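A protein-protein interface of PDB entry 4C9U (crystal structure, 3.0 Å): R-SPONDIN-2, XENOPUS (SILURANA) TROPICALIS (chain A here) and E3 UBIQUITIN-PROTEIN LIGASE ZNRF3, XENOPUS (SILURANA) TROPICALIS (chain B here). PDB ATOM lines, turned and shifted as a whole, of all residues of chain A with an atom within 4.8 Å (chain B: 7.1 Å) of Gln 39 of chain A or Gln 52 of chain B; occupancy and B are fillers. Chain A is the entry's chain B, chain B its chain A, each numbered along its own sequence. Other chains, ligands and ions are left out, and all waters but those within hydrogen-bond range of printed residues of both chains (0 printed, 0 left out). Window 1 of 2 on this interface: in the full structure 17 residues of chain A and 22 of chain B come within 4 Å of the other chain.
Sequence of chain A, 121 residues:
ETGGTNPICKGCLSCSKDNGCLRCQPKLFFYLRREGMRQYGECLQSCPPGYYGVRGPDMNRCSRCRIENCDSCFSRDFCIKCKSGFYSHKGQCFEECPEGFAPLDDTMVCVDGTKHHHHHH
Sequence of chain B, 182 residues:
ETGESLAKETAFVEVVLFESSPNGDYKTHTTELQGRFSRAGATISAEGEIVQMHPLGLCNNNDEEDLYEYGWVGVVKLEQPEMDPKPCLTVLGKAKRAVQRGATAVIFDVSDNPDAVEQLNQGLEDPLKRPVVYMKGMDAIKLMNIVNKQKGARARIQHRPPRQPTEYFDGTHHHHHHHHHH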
ATOM      1  N   ASP A  18      32.037  21.515  -7.830  1.00  0.00           N
ATOM      2  CA  ASP A  18      30.897  20.761  -7.382  1.00  0.00           C
ATOM      3  C   ASP A  18      29.850  20.476  -8.472  1.00  0.00           C
ATOM      4  O   ASP A  18      29.109  19.489  -8.377  1.00  0.00           O
ATOM      5  CB  ASP A  18      30.274  21.422  -6.121  1.00  0.00           C
ATOM      6  CG  ASP A  18      30.665  20.728  -4.815  1.00  0.00           C
ATOM      7  OD1 ASP A  18      31.044  19.537  -4.886  1.00  0.00           O
ATOM      8  OD2 ASP A  18      30.543  21.355  -3.725  1.00  0.00           O
ATOM      9  N   ASN A  19      29.788  21.319  -9.497  1.00  0.00           N
ATOM     10  CA  ASN A  19      28.808  21.176 -10.568  1.00  0.00           C
ATOM     11  C   ASN A  19      29.410  20.860 -11.958  1.00  0.00           C
ATOM     12  O   ASN A  19      28.684  20.651 -12.926  1.00  0.00           O
ATOM     13  CB  ASN A  19      27.955  22.460 -10.641  1.00  0.00           C
ATOM     14  CG  ASN A  19      26.904  22.587  -9.510  1.00  0.00           C
ATOM     15  OD1 ASN A  19      25.992  21.745  -9.322  1.00  0.00           O
ATOM     16  ND2 ASN A  19      26.992  23.695  -8.798  1.00  0.00           N
ATOM     17  N   LEU A  32      24.479  16.615 -19.097  1.00  0.00           N
ATOM     18  CA  LEU A  32      24.425  16.415 -17.672  1.00  0.00           C
ATOM     19  C   LEU A  32      24.660  14.953 -17.316  1.00  0.00           C
ATOM     20  O   LEU A  32      23.776  14.110 -17.437  1.00  0.00           O
ATOM     21  CB  LEU A  32      23.079  16.850 -17.177  1.00  0.00           C
ATOM     22  CG  LEU A  32      22.843  18.349 -17.248  1.00  0.00           C
ATOM     23  CD1 LEU A  32      21.386  18.685 -17.013  1.00  0.00           C
ATOM     24  CD2 LEU A  32      23.719  19.064 -16.237  1.00  0.00           C
ATOM     25  N   ARG A  33      25.879  14.649 -16.913  1.00  0.00           N
ATOM     26  CA  ARG A  33      26.232  13.304 -16.575  1.00  0.00           C
ATOM     27  C   ARG A  33      25.725  13.087 -15.190  1.00  0.00           C
ATOM     28  O   ARG A  33      26.081  13.828 -14.314  1.00  0.00           O
ATOM     29  CB  ARG A  33      27.756  13.081 -16.621  1.00  0.00           C
ATOM     30  CG  ARG A  33      28.176  11.661 -16.226  1.00  0.00           C
ATOM     31  CD  ARG A  33      29.658  11.387 -16.435  1.00  0.00           C
ATOM     32  NE  ARG A  33      29.977  11.018 -17.800  1.00  0.00           N
ATOM     33  CZ  ARG A  33      29.696   9.842 -18.365  1.00  0.00           C
ATOM     34  NH1 ARG A  33      29.069   8.878 -17.688  1.00  0.00           N
ATOM     35  NH2 ARG A  33      30.035   9.634 -19.635  1.00  0.00           N
ATOM     36  N   ARG A  34      24.909  12.054 -15.026  1.00  0.00           N
ATOM     37  CA  ARG A  34      24.431  11.583 -13.746  1.00  0.00           C
ATOM     38  C   ARG A  34      25.339  10.435 -13.361  1.00  0.00           C
ATOM     39  O   ARG A  34      25.624   9.579 -14.164  1.00  0.00           O
ATOM     40  CB  ARG A  34      22.993  11.103 -13.932  1.00  0.00           C
ATOM     41  CG  ARG A  34      22.287  10.331 -12.815  1.00  0.00           C
ATOM     42  CD  ARG A  34      21.236  11.208 -12.183  1.00  0.00           C
ATOM     43  NE  ARG A  34      21.768  11.938 -11.050  1.00  0.00           N
ATOM     44  CZ  ARG A  34      21.280  13.088 -10.609  1.00  0.00           C
ATOM     45  NH1 ARG A  34      20.255  13.686 -11.209  1.00  0.00           N
ATOM     46  NH2 ARG A  34      21.846  13.653  -9.562  1.00  0.00           N
ATOM     47  N   MET A  37      24.530   9.933  -6.853  1.00  0.00           N
ATOM     48  CA  MET A  37      23.869  11.149  -6.394  1.00  0.00           C
ATOM     49  C   MET A  37      24.326  12.351  -7.189  1.00  0.00           C
ATOM     50  O   MET A  37      23.643  13.370  -7.184  1.00  0.00           O
ATOM     51  CB  MET A  37      24.165  11.446  -4.935  1.00  0.00           C
ATOM     52  CG  MET A  37      23.687  10.405  -3.948  1.00  0.00           C
ATOM     53  SD  MET A  37      24.730  10.340  -2.462  1.00  0.00           S
ATOM     54  CE  MET A  37      23.866  11.511  -1.429  1.00  0.00           C
ATOM     55  N   ARG A  38      25.472  12.260  -7.862  1.00  0.00           N
ATOM     56  CA  ARG A  38      26.039  13.443  -8.513  1.00  0.00           C
ATOM     57  C   ARG A  38      25.357  13.728  -9.830  1.00  0.00           C
ATOM     58  O   ARG A  38      24.717  12.845 -10.413  1.00  0.00           O
ATOM     59  CB  ARG A  38      27.507  13.262  -8.806  1.00  0.00           C
ATOM     60  CG  ARG A  38      28.327  13.009  -7.586  1.00  0.00           C
ATOM     61  CD  ARG A  38      29.766  12.755  -7.986  1.00  0.00           C
ATOM     62  NE  ARG A  38      30.374  13.926  -8.610  1.00  0.00           N
ATOM     63  CZ  ARG A  38      31.569  13.931  -9.195  1.00  0.00           C
ATOM     64  NH1 ARG A  38      32.296  12.819  -9.276  1.00  0.00           N
ATOM     65  NH2 ARG A  38      32.027  15.059  -9.726  1.00  0.00           N
ATOM     66  N   GLN A  39      25.515  14.958 -10.297  1.00  0.00           N
ATOM     67  CA  GLN A  39      25.144  15.334 -11.654  1.00  0.00           C
ATOM     68  C   GLN A  39      25.978  16.526 -11.989  1.00  0.00           C
ATOM     69  O   GLN A  39      25.996  17.502 -11.225  1.00  0.00           O
ATOM     70  CB  GLN A  39      23.663  15.698 -11.746  1.00  0.00           C
ATOM     71  CG  GLN A  39      23.238  16.225 -13.087  1.00  0.00           C
ATOM     72  CD  GLN A  39      21.802  16.696 -13.118  1.00  0.00           C
ATOM     73  OE1 GLN A  39      21.375  17.557 -12.336  1.00  0.00           O
ATOM     74  NE2 GLN A  39      21.027  16.122 -14.017  1.00  0.00           N
ATOM     75  N   TYR A  40      26.696  16.484 -13.098  1.00  0.00           N
ATOM     76  CA  TYR A  40      27.584  17.600 -13.411  1.00  0.00           C
ATOM     77  C   TYR A  40      27.705  17.879 -14.902  1.00  0.00           C
ATOM     78  O   TYR A  40      27.320  17.070 -15.741  1.00  0.00           O
ATOM     79  CB  TYR A  40      28.951  17.388 -12.755  1.00  0.00           C
ATOM     80  CG  TYR A  40      29.624  16.121 -13.162  1.00  0.00           C
ATOM     81  CD1 TYR A  40      30.326  16.053 -14.362  1.00  0.00           C
ATOM     82  CD2 TYR A  40      29.549  14.988 -12.366  1.00  0.00           C
ATOM     83  CE1 TYR A  40      30.950  14.888 -14.773  1.00  0.00           C
ATOM     84  CE2 TYR A  40      30.160  13.808 -12.761  1.00  0.00           C
ATOM     85  CZ  TYR A  40      30.866  13.755 -13.974  1.00  0.00           C
ATOM     86  OH  TYR A  40      31.525  12.602 -14.410  1.00  0.00           O
ATOM     87  N   GLY A  41      28.216  19.057 -15.228  1.00  0.00           N
ATOM     88  CA  GLY A  41      28.279  19.481 -16.614  1.00  0.00           C
ATOM     89  C   GLY A  41      29.434  18.872 -17.356  1.00  0.00           C
ATOM     90  O   GLY A  41      30.485  18.680 -16.789  1.00  0.00           O
ATOM     91  N   ILE B  50      18.937  11.451  -1.500  1.00  0.00           N
ATOM     92  CA  ILE B  50      19.497  12.687  -1.969  1.00  0.00           C
ATOM     93  C   ILE B  50      19.849  12.566  -3.453  1.00  0.00           C
ATOM     94  O   ILE B  50      20.279  11.498  -3.920  1.00  0.00           O
ATOM     95  CB  ILE B  50      20.778  13.012  -1.211  1.00  0.00           C
ATOM     96  CG1 ILE B  50      20.461  13.392   0.227  1.00  0.00           C
ATOM     97  CG2 ILE B  50      21.561  14.126  -1.894  1.00  0.00           C
ATOM     98  CD1 ILE B  50      21.664  13.306   1.143  1.00  0.00           C
ATOM     99  N   VAL B  51      19.685  13.665  -4.187  1.00  0.00           N
ATOM    100  CA  VAL B  51      20.006  13.711  -5.597  1.00  0.00           C
ATOM    101  C   VAL B  51      20.510  15.115  -5.887  1.00  0.00           C
ATOM    102  O   VAL B  51      19.734  16.082  -5.819  1.00  0.00           O
ATOM    103  CB  VAL B  51      18.733  13.505  -6.452  1.00  0.00           C
ATOM    104  CG1 VAL B  51      19.018  13.747  -7.917  1.00  0.00           C
ATOM    105  CG2 VAL B  51      18.146  12.133  -6.260  1.00  0.00           C
ATOM    106  N   GLN B  52      21.775  15.244  -6.253  1.00  0.00           N
ATOM    107  CA  GLN B  52      22.249  16.529  -6.723  1.00  0.00           C
ATOM    108  C   GLN B  52      21.532  16.957  -8.014  1.00  0.00           C
ATOM    109  O   GLN B  52      21.214  16.124  -8.852  1.00  0.00           O
ATOM    110  CB  GLN B  52      23.737  16.481  -7.017  1.00  0.00           C
ATOM    111  CG  GLN B  52      24.311  17.852  -7.361  1.00  0.00           C
ATOM    112  CD  GLN B  52      25.800  17.793  -7.599  1.00  0.00           C
ATOM    113  OE1 GLN B  52      26.359  16.730  -7.880  1.00  0.00           O
ATOM    114  NE2 GLN B  52      26.443  18.944  -7.524  1.00  0.00           N
ATOM    115  N   MET B  53      21.288  18.254  -8.168  1.00  0.00           N
ATOM    116  CA  MET B  53      20.831  18.779  -9.429  1.00  0.00           C
ATOM    117  C   MET B  53      21.698  19.951  -9.802  1.00  0.00           C
ATOM    118  O   MET B  53      21.814  20.905  -9.064  1.00  0.00           O
ATOM    119  CB  MET B  53      19.384  19.242  -9.364  1.00  0.00           C
ATOM    120  CG  MET B  53      18.388  18.181  -8.978  1.00  0.00           C
ATOM    121  SD  MET B  53      18.155  16.871 -10.217  1.00  0.00           S
ATOM    122  CE  MET B  53      16.819  17.509 -11.216  1.00  0.00           C
ATOM    123  N   HIS B  54      22.305  19.890 -10.958  1.00  0.00           N
ATOM    124  CA  HIS B  54      22.939  21.047 -11.529  1.00  0.00           C
ATOM    125  C   HIS B  54      21.897  22.170 -11.656  1.00  0.00           C
ATOM    126  O   HIS B  54      20.772  21.903 -12.107  1.00  0.00           O
ATOM    127  CB  HIS B  54      23.451  20.655 -12.909  1.00  0.00           C
ATOM    128  CG  HIS B  54      24.521  21.532 -13.449  1.00  0.00           C
ATOM    129  ND1 HIS B  54      24.259  22.746 -14.038  1.00  0.00           N
ATOM    130  CD2 HIS B  54      25.856  21.337 -13.558  1.00  0.00           C
ATOM    131  CE1 HIS B  54      25.393  23.283 -14.456  1.00  0.00           C
ATOM    132  NE2 HIS B  54      26.381  22.447 -14.174  1.00  0.00           N
ATOM    133  N   PRO B  55      22.260  23.421 -11.276  1.00  0.00           N
ATOM    134  CA  PRO B  55      21.338  24.545 -11.342  1.00  0.00           C
ATOM    135  C   PRO B  55      20.831  24.887 -12.748  1.00  0.00           C
ATOM    136  O   PRO B  55      19.759  25.501 -12.877  1.00  0.00           O
ATOM    137  CB  PRO B  55      22.123  25.674 -10.729  1.00  0.00           C
ATOM    138  CG  PRO B  55      23.541  25.321 -10.981  1.00  0.00           C
ATOM    139  CD  PRO B  55      23.595  23.849 -10.829  1.00  0.00           C
ATOM    140  N   LEU B  56      21.522  24.454 -13.796  1.00  0.00           N
ATOM    141  CA  LEU B  56      20.922  24.454 -15.154  1.00  0.00           C
ATOM    142  C   LEU B  56      20.165  23.189 -15.559  1.00  0.00           C
ATOM    143  O   LEU B  56      19.717  23.075 -16.686  1.00  0.00           O
ATOM    144  CB  LEU B  56      21.989  24.730 -16.203  1.00  0.00           C
ATOM    145  CG  LEU B  56      22.647  26.094 -16.034  1.00  0.00           C
ATOM    146  CD1 LEU B  56      23.549  26.339 -17.237  1.00  0.00           C
ATOM    147  CD2 LEU B  56      21.614  27.216 -15.874  1.00  0.00           C
ATOM    148  N   GLY B  57      20.044  22.230 -14.658  1.00  0.00           N
ATOM    149  CA  GLY B  57      19.207  21.070 -14.900  1.00  0.00           C
ATOM    150  C   GLY B  57      17.757  21.464 -14.755  1.00  0.00           C
ATOM    151  O   GLY B  57      16.866  20.785 -15.246  1.00  0.00           O
ATOM    152  N   LEU B  58      17.534  22.570 -14.062  1.00  0.00           N
ATOM    153  CA  LEU B  58      16.212  22.982 -13.706  1.00  0.00           C
ATOM    154  C   LEU B  58      15.794  24.168 -14.529  1.00  0.00           C
ATOM    155  O   LEU B  58      15.926  25.310 -14.100  1.00  0.00           O
ATOM    156  CB  LEU B  58      16.214  23.354 -12.243  1.00  0.00           C
ATOM    157  CG  LEU B  58      16.581  22.173 -11.358  1.00  0.00           C
ATOM    158  CD1 LEU B  58      16.855  22.688  -9.967  1.00  0.00           C
ATOM    159  CD2 LEU B  58      15.458  21.148 -11.345  1.00  0.00           C
ATOM    160  N   ASP B  66      14.636  13.099 -17.606  1.00  0.00           N
ATOM    161  CA  ASP B  66      14.528  11.792 -16.992  1.00  0.00           C
ATOM    162  C   ASP B  66      13.481  11.797 -15.889  1.00  0.00           C
ATOM    163  O   ASP B  66      13.293  12.797 -15.181  1.00  0.00           O
ATOM    164  CB  ASP B  66      15.881  11.323 -16.428  1.00  0.00           C
ATOM    165  CG  ASP B  66      16.839  10.774 -17.509  1.00  0.00           C
ATOM    166  OD1 ASP B  66      16.396  10.101 -18.451  1.00  0.00           O
ATOM    167  OD2 ASP B  66      18.061  10.982 -17.409  1.00  0.00           O
ATOM    168  N   TYR B  68      12.791  10.693 -12.463  1.00  0.00           N
ATOM    169  CA  TYR B  68      13.398  10.259 -11.215  1.00  0.00           C
ATOM    170  C   TYR B  68      12.260   9.744 -10.349  1.00  0.00           C
ATOM    171  O   TYR B  68      11.142  10.276 -10.407  1.00  0.00           O
ATOM    172  CB  TYR B  68      14.145  11.402 -10.513  1.00  0.00           C
ATOM    173  CG  TYR B  68      15.319  11.969 -11.298  1.00  0.00           C
ATOM    174  CD1 TYR B  68      16.075  11.158 -12.129  1.00  0.00           C
ATOM    175  CD2 TYR B  68      15.684  13.315 -11.186  1.00  0.00           C
ATOM    176  CE1 TYR B  68      17.150  11.671 -12.843  1.00  0.00           C
ATOM    177  CE2 TYR B  68      16.757  13.839 -11.893  1.00  0.00           C
ATOM    178  CZ  TYR B  68      17.491  13.014 -12.728  1.00  0.00           C
ATOM    179  OH  TYR B  68      18.579  13.479 -13.452  1.00  0.00           O
ATOM    180  N   TRP B  72      12.394  12.201  -3.998  1.00  0.00           N
ATOM    181  CA  TRP B  72      13.808  12.460  -3.817  1.00  0.00           C
ATOM    182  C   TRP B  72      13.997  13.793  -3.136  1.00  0.00           C
ATOM    183  O   TRP B  72      13.117  14.649  -3.191  1.00  0.00           O
ATOM    184  CB  TRP B  72      14.551  12.431  -5.149  1.00  0.00           C
ATOM    185  CG  TRP B  72      13.957  13.207  -6.238  1.00  0.00           C
ATOM    186  CD1 TRP B  72      12.953  12.817  -7.046  1.00  0.00           C
ATOM    187  CD2 TRP B  72      14.347  14.494  -6.673  1.00  0.00           C
ATOM    188  NE1 TRP B  72      12.662  13.803  -7.950  1.00  0.00           N
ATOM    189  CE2 TRP B  72      13.529  14.837  -7.745  1.00  0.00           C
ATOM    190  CE3 TRP B  72      15.304  15.391  -6.257  1.00  0.00           C
ATOM    191  CZ2 TRP B  72      13.633  16.029  -8.396  1.00  0.00           C
ATOM    192  CZ3 TRP B  72      15.415  16.595  -6.919  1.00  0.00           C
ATOM    193  CH2 TRP B  72      14.579  16.909  -7.966  1.00  0.00           C
ATOM    194  N   VAL B  73      15.136  13.981  -2.490  1.00  0.00           N
ATOM    195  CA  VAL B  73      15.484  15.263  -1.887  1.00  0.00           C
ATOM    196  C   VAL B  73      16.567  15.916  -2.717  1.00  0.00           C
ATOM    197  O   VAL B  73      17.693  15.391  -2.848  1.00  0.00           O
ATOM    198  CB  VAL B  73      16.026  15.081  -0.466  1.00  0.00           C
ATOM    199  CG1 VAL B  73      16.429  16.412   0.130  1.00  0.00           C
ATOM    200  CG2 VAL B  73      14.991  14.378   0.409  1.00  0.00           C
ATOM    201  N   GLY B  74      16.255  17.083  -3.255  1.00  0.00           N
ATOM    202  CA  GLY B  74      17.167  17.733  -4.180  1.00  0.00           C
ATOM    203  C   GLY B  74      18.266  18.435  -3.401  1.00  0.00           C
ATOM    204  O   GLY B  74      18.036  18.961  -2.320  1.00  0.00           O
ATOM    205  N   VAL B  75      19.472  18.416  -3.925  1.00  0.00           N
ATOM    206  CA  VAL B  75      20.533  19.247  -3.393  1.00  0.00           C
ATOM    207  C   VAL B  75      21.165  20.006  -4.524  1.00  0.00           C
ATOM    208  O   VAL B  75      21.648  19.406  -5.491  1.00  0.00           O
ATOM    209  CB  VAL B  75      21.601  18.382  -2.785  1.00  0.00           C
ATOM    210  CG1 VAL B  75      22.775  19.210  -2.348  1.00  0.00           C
ATOM    211  CG2 VAL B  75      21.006  17.618  -1.633  1.00  0.00           C
ATOM    212  N   VAL B  76      21.151  21.326  -4.412  1.00  0.00           N
ATOM    213  CA  VAL B  76      21.567  22.216  -5.489  1.00  0.00           C
ATOM    214  C   VAL B  76      22.602  23.165  -4.917  1.00  0.00           C
ATOM    215  O   VAL B  76      22.389  23.741  -3.832  1.00  0.00           O
ATOM    216  CB  VAL B  76      20.375  23.041  -5.967  1.00  0.00           C
ATOM    217  CG1 VAL B  76      20.762  23.943  -7.097  1.00  0.00           C
ATOM    218  CG2 VAL B  76      19.276  22.131  -6.383  1.00  0.00           C
ATOM    219  N   LYS B  77      23.706  23.344  -5.631  1.00  0.00           N
ATOM    220  CA  LYS B  77      24.739  24.298  -5.208  1.00  0.00           C
ATOM    221  C   LYS B  77      24.764  25.473  -6.168  1.00  0.00           C
ATOM    222  O   LYS B  77      24.998  25.287  -7.351  1.00  0.00           O
ATOM    223  CB  LYS B  77      26.076  23.624  -5.212  1.00  0.00           C
ATOM    224  CG  LYS B  77      27.133  24.591  -4.864  1.00  0.00           C
ATOM    225  CD  LYS B  77      28.365  23.851  -4.391  1.00  0.00           C
ATOM    226  CE  LYS B  77      29.199  24.719  -3.477  1.00  0.00           C
ATOM    227  NZ  LYS B  77      29.380  26.058  -4.094  1.00  0.00           N
ATOM    228  N   ARG B 101       9.146  17.666 -10.588  1.00  0.00           N
ATOM    229  CA  ARG B 101       9.822  16.472 -11.019  1.00  0.00           C
ATOM    230  C   ARG B 101       9.993  15.406  -9.911  1.00  0.00           C
ATOM    231  O   ARG B 101      10.702  14.403 -10.088  1.00  0.00           O
ATOM    232  CB  ARG B 101      11.146  16.855 -11.642  1.00  0.00           C
ATOM    233  CG  ARG B 101      10.955  17.701 -12.899  1.00  0.00           C
ATOM    234  CD  ARG B 101      12.268  18.082 -13.576  1.00  0.00           C
ATOM    235  NE  ARG B 101      13.060  16.908 -13.862  1.00  0.00           N
ATOM    236  CZ  ARG B 101      14.343  16.926 -14.218  1.00  0.00           C
ATOM    237  NH1 ARG B 101      15.008  18.073 -14.370  1.00  0.00           N
ATOM    238  NH2 ARG B 101      14.968  15.771 -14.437  1.00  0.00           N
ATOM    239  N   MET B 144      28.195  18.569   0.657  1.00  0.00           N
ATOM    240  CA  MET B 144      28.707  18.384  -0.706  1.00  0.00           C
ATOM    241  C   MET B 144      29.723  17.261  -0.829  1.00  0.00           C
ATOM    242  O   MET B 144      29.861  16.662  -1.896  1.00  0.00           O
ATOM    243  CB  MET B 144      29.293  19.692  -1.263  1.00  0.00           C
ATOM    244  CG  MET B 144      28.272  20.820  -1.388  1.00  0.00           C
ATOM    245  SD  MET B 144      26.629  20.379  -2.044  1.00  0.00           S
ATOM    246  CE  MET B 144      27.040  19.574  -3.611  1.00  0.00           C
ATOM    247  N   VAL B 147      27.790  13.887  -0.999  1.00  0.00           N
ATOM    248  CA  VAL B 147      27.272  13.789  -2.338  1.00  0.00           C
ATOM    249  C   VAL B 147      28.390  13.319  -3.246  1.00  0.00           C
ATOM    250  O   VAL B 147      28.216  12.405  -4.051  1.00  0.00           O
ATOM    251  CB  VAL B 147      26.790  15.163  -2.810  1.00  0.00           C
ATOM    252  CG1 VAL B 147      26.471  15.145  -4.301  1.00  0.00           C
ATOM    253  CG2 VAL B 147      25.573  15.605  -2.007  1.00  0.00           C
ATOM    254  N   ASN B 148      29.550  13.932  -3.078  1.00  0.00           N
ATOM    255  CA  ASN B 148      30.671  13.650  -3.933  1.00  0.00           C
ATOM    256  C   ASN B 148      31.331  12.302  -3.818  1.00  0.00           C
ATOM    257  O   ASN B 148      31.815  11.797  -4.813  1.00  0.00           O
ATOM    258  CB  ASN B 148      31.702  14.761  -3.784  1.00  0.00           C
ATOM    259  CG  ASN B 148      31.419  15.918  -4.744  1.00  0.00           C
ATOM    260  OD1 ASN B 148      30.294  16.479  -4.787  1.00  0.00           O
ATOM    261  ND2 ASN B 148      32.422  16.279  -5.520  1.00  0.00           N
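Of the 10 printed residues of chain A, 8 touch a printed residue of chain B. Hydrophobic or aromatic side chains of chain A within 4 Å of the printed part of chain B: Leu 32 and Met 37. Of the 21 printed residues of chain B, 12 touch a printed residue of chain A. Among the printed residues, 25 pairs touch across the chains. Among the printed residues, no Asp or Glu carboxylate lies within 4 Å of a Lys or Arg side-chain nitrogen of the other chain.
A ring nitrogen (ND1) of His 54 of chain B sits close to the backbone NH (N) of Leu 56 of chain B. N of Val 75 of chain B sits at hydrogen-bond distance from O of Val 51 of chain B (3.0 Å). O of Gly 57 of chain B lies within hydrogen-bond range of NH1 of Arg 101 of chain B (3.4 Å). O of Asn 19 of chain A sits at hydrogen-bond distance from N of Gly 41 of chain A (2.8 Å). N of Val 51 of chain B is in hydrogen-bond range of O of Val 73 of chain B, 3.0 Å away. N of Met 53 of chain B lies within hydrogen-bond range of O of Val 75 of chain B, 2.9 Å away.
Among the printed residues, merely in contact across the chains: Asp 18 of chain A with Lys 77 of chain B (3.4 Å), Asp 18 of chain A with Met 144 of chain B (3.2 Å), Asn 19 of chain A with Pro 55 of chain B (3.5 Å), Leu 32 of chain A with His 54 of chain B (3.7 Å), Leu 32 of chain A with Gly 57 of chain B (3.9 Å), Arg 34 of chain A with Val 51 of chain B (3.3 Å), Arg 34 of chain A with Met 53 of chain B (3.9 Å), Met 37 of chain A with Ile 50 of chain B (3.4 Å), Met 37 of chain A with Val 51 of chain B (3.8 Å), Arg 38 of chain A with Gln 52 of chain B (3.4 Å), Arg 38 of chain A with Val 147 of chain B (3.6 Å), Arg 38 of chain A with Asn 148 of chain B (3.9 Å), Gln 39 of chain A with Met 53 of chain B (3.2 Å), Gln 39 of chain A with Tyr 68 of chain B (3.6 Å) and Gly 41 of chain A with His 54 of chain B (3.7 Å).
Printed residues of chain B within 4 Å of Asn 19 of chain A: Gln 52, His 54, Pro 55 and Lys 77. Of the printed residues of chain B, Arg 34 of chain A touches Val 51 (3.3 Å), Gln 52 (2.6 Å), Met 53 (3.9 Å) and Tyr 68 (2.8 Å). Of chain B, only Gln 52, Met 53, His 54 and Tyr 68 come within 4 Å of Gln 39 of chain A. Tyr 40 of chain A touches none of the printed residues of chain B. Of chain A, only Asp 18, Asn 19, Arg 34, Met 37, Arg 38 and Gln 39 come within 4 Å of Gln 52 of chain B. Printed residues of chain A within 4 Å of His 54 of chain B: Asn 19, Leu 32, Gln 39 and Gly 41. Val 76 of chain B touches none of the printed residues of chain A. Of the printed residues of chain A, Met 144 of chain B touches Asp 18. The nearest residue of chain B that does not touch Gln 39 of chain A is Gly 57 of chain B (4.9 Å).
NE2 of Gln 52 of chain B lies within hydrogen-bond range of OD1 of Asn 19 of chain A, at 3.4 Å. O of Asn 19 of chain A sits close to NE2 of His 54 of chain B (3.2 Å). The side-chain carboxylate (OD1) of Asp 18 of chain A lies close to the side-chain amide oxygen (OD1) of Asn 148 of chain B (3.2 Å). N of Gln 52 of chain B is in hydrogen-bond range of O of Met 37 of chain A (2.8 Å). N of His 54 of chain B is in hydrogen-bond range of OE1 of Gln 39 of chain A. The backbone carbonyl oxygen (O) of Lys 77 of chain B sits at hydrogen-bond distance from the side-chain amide nitrogen (ND2) of Asn 19 of chain A (2.9 Å). The side-chain hydroxyl of Tyr 68 of chain B is in hydrogen-bond range of the guanidinium group of Arg 34 of chain A (2.8 Å). OE1 of Gln 52 of chain B sits at hydrogen-bond distance from N of Gln 39 of chain A (3.1 Å). The side-chain amide nitrogen of Gln 52 of chain B lies within hydrogen-bond range of the backbone carbonyl oxygen of Asp 18 of chain A. The backbone carbonyl oxygen (O) of Gln 52 of chain B lies within hydrogen-bond range of the guanidinium group (NH2) of Arg 34 of chain A (2.6 Å).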
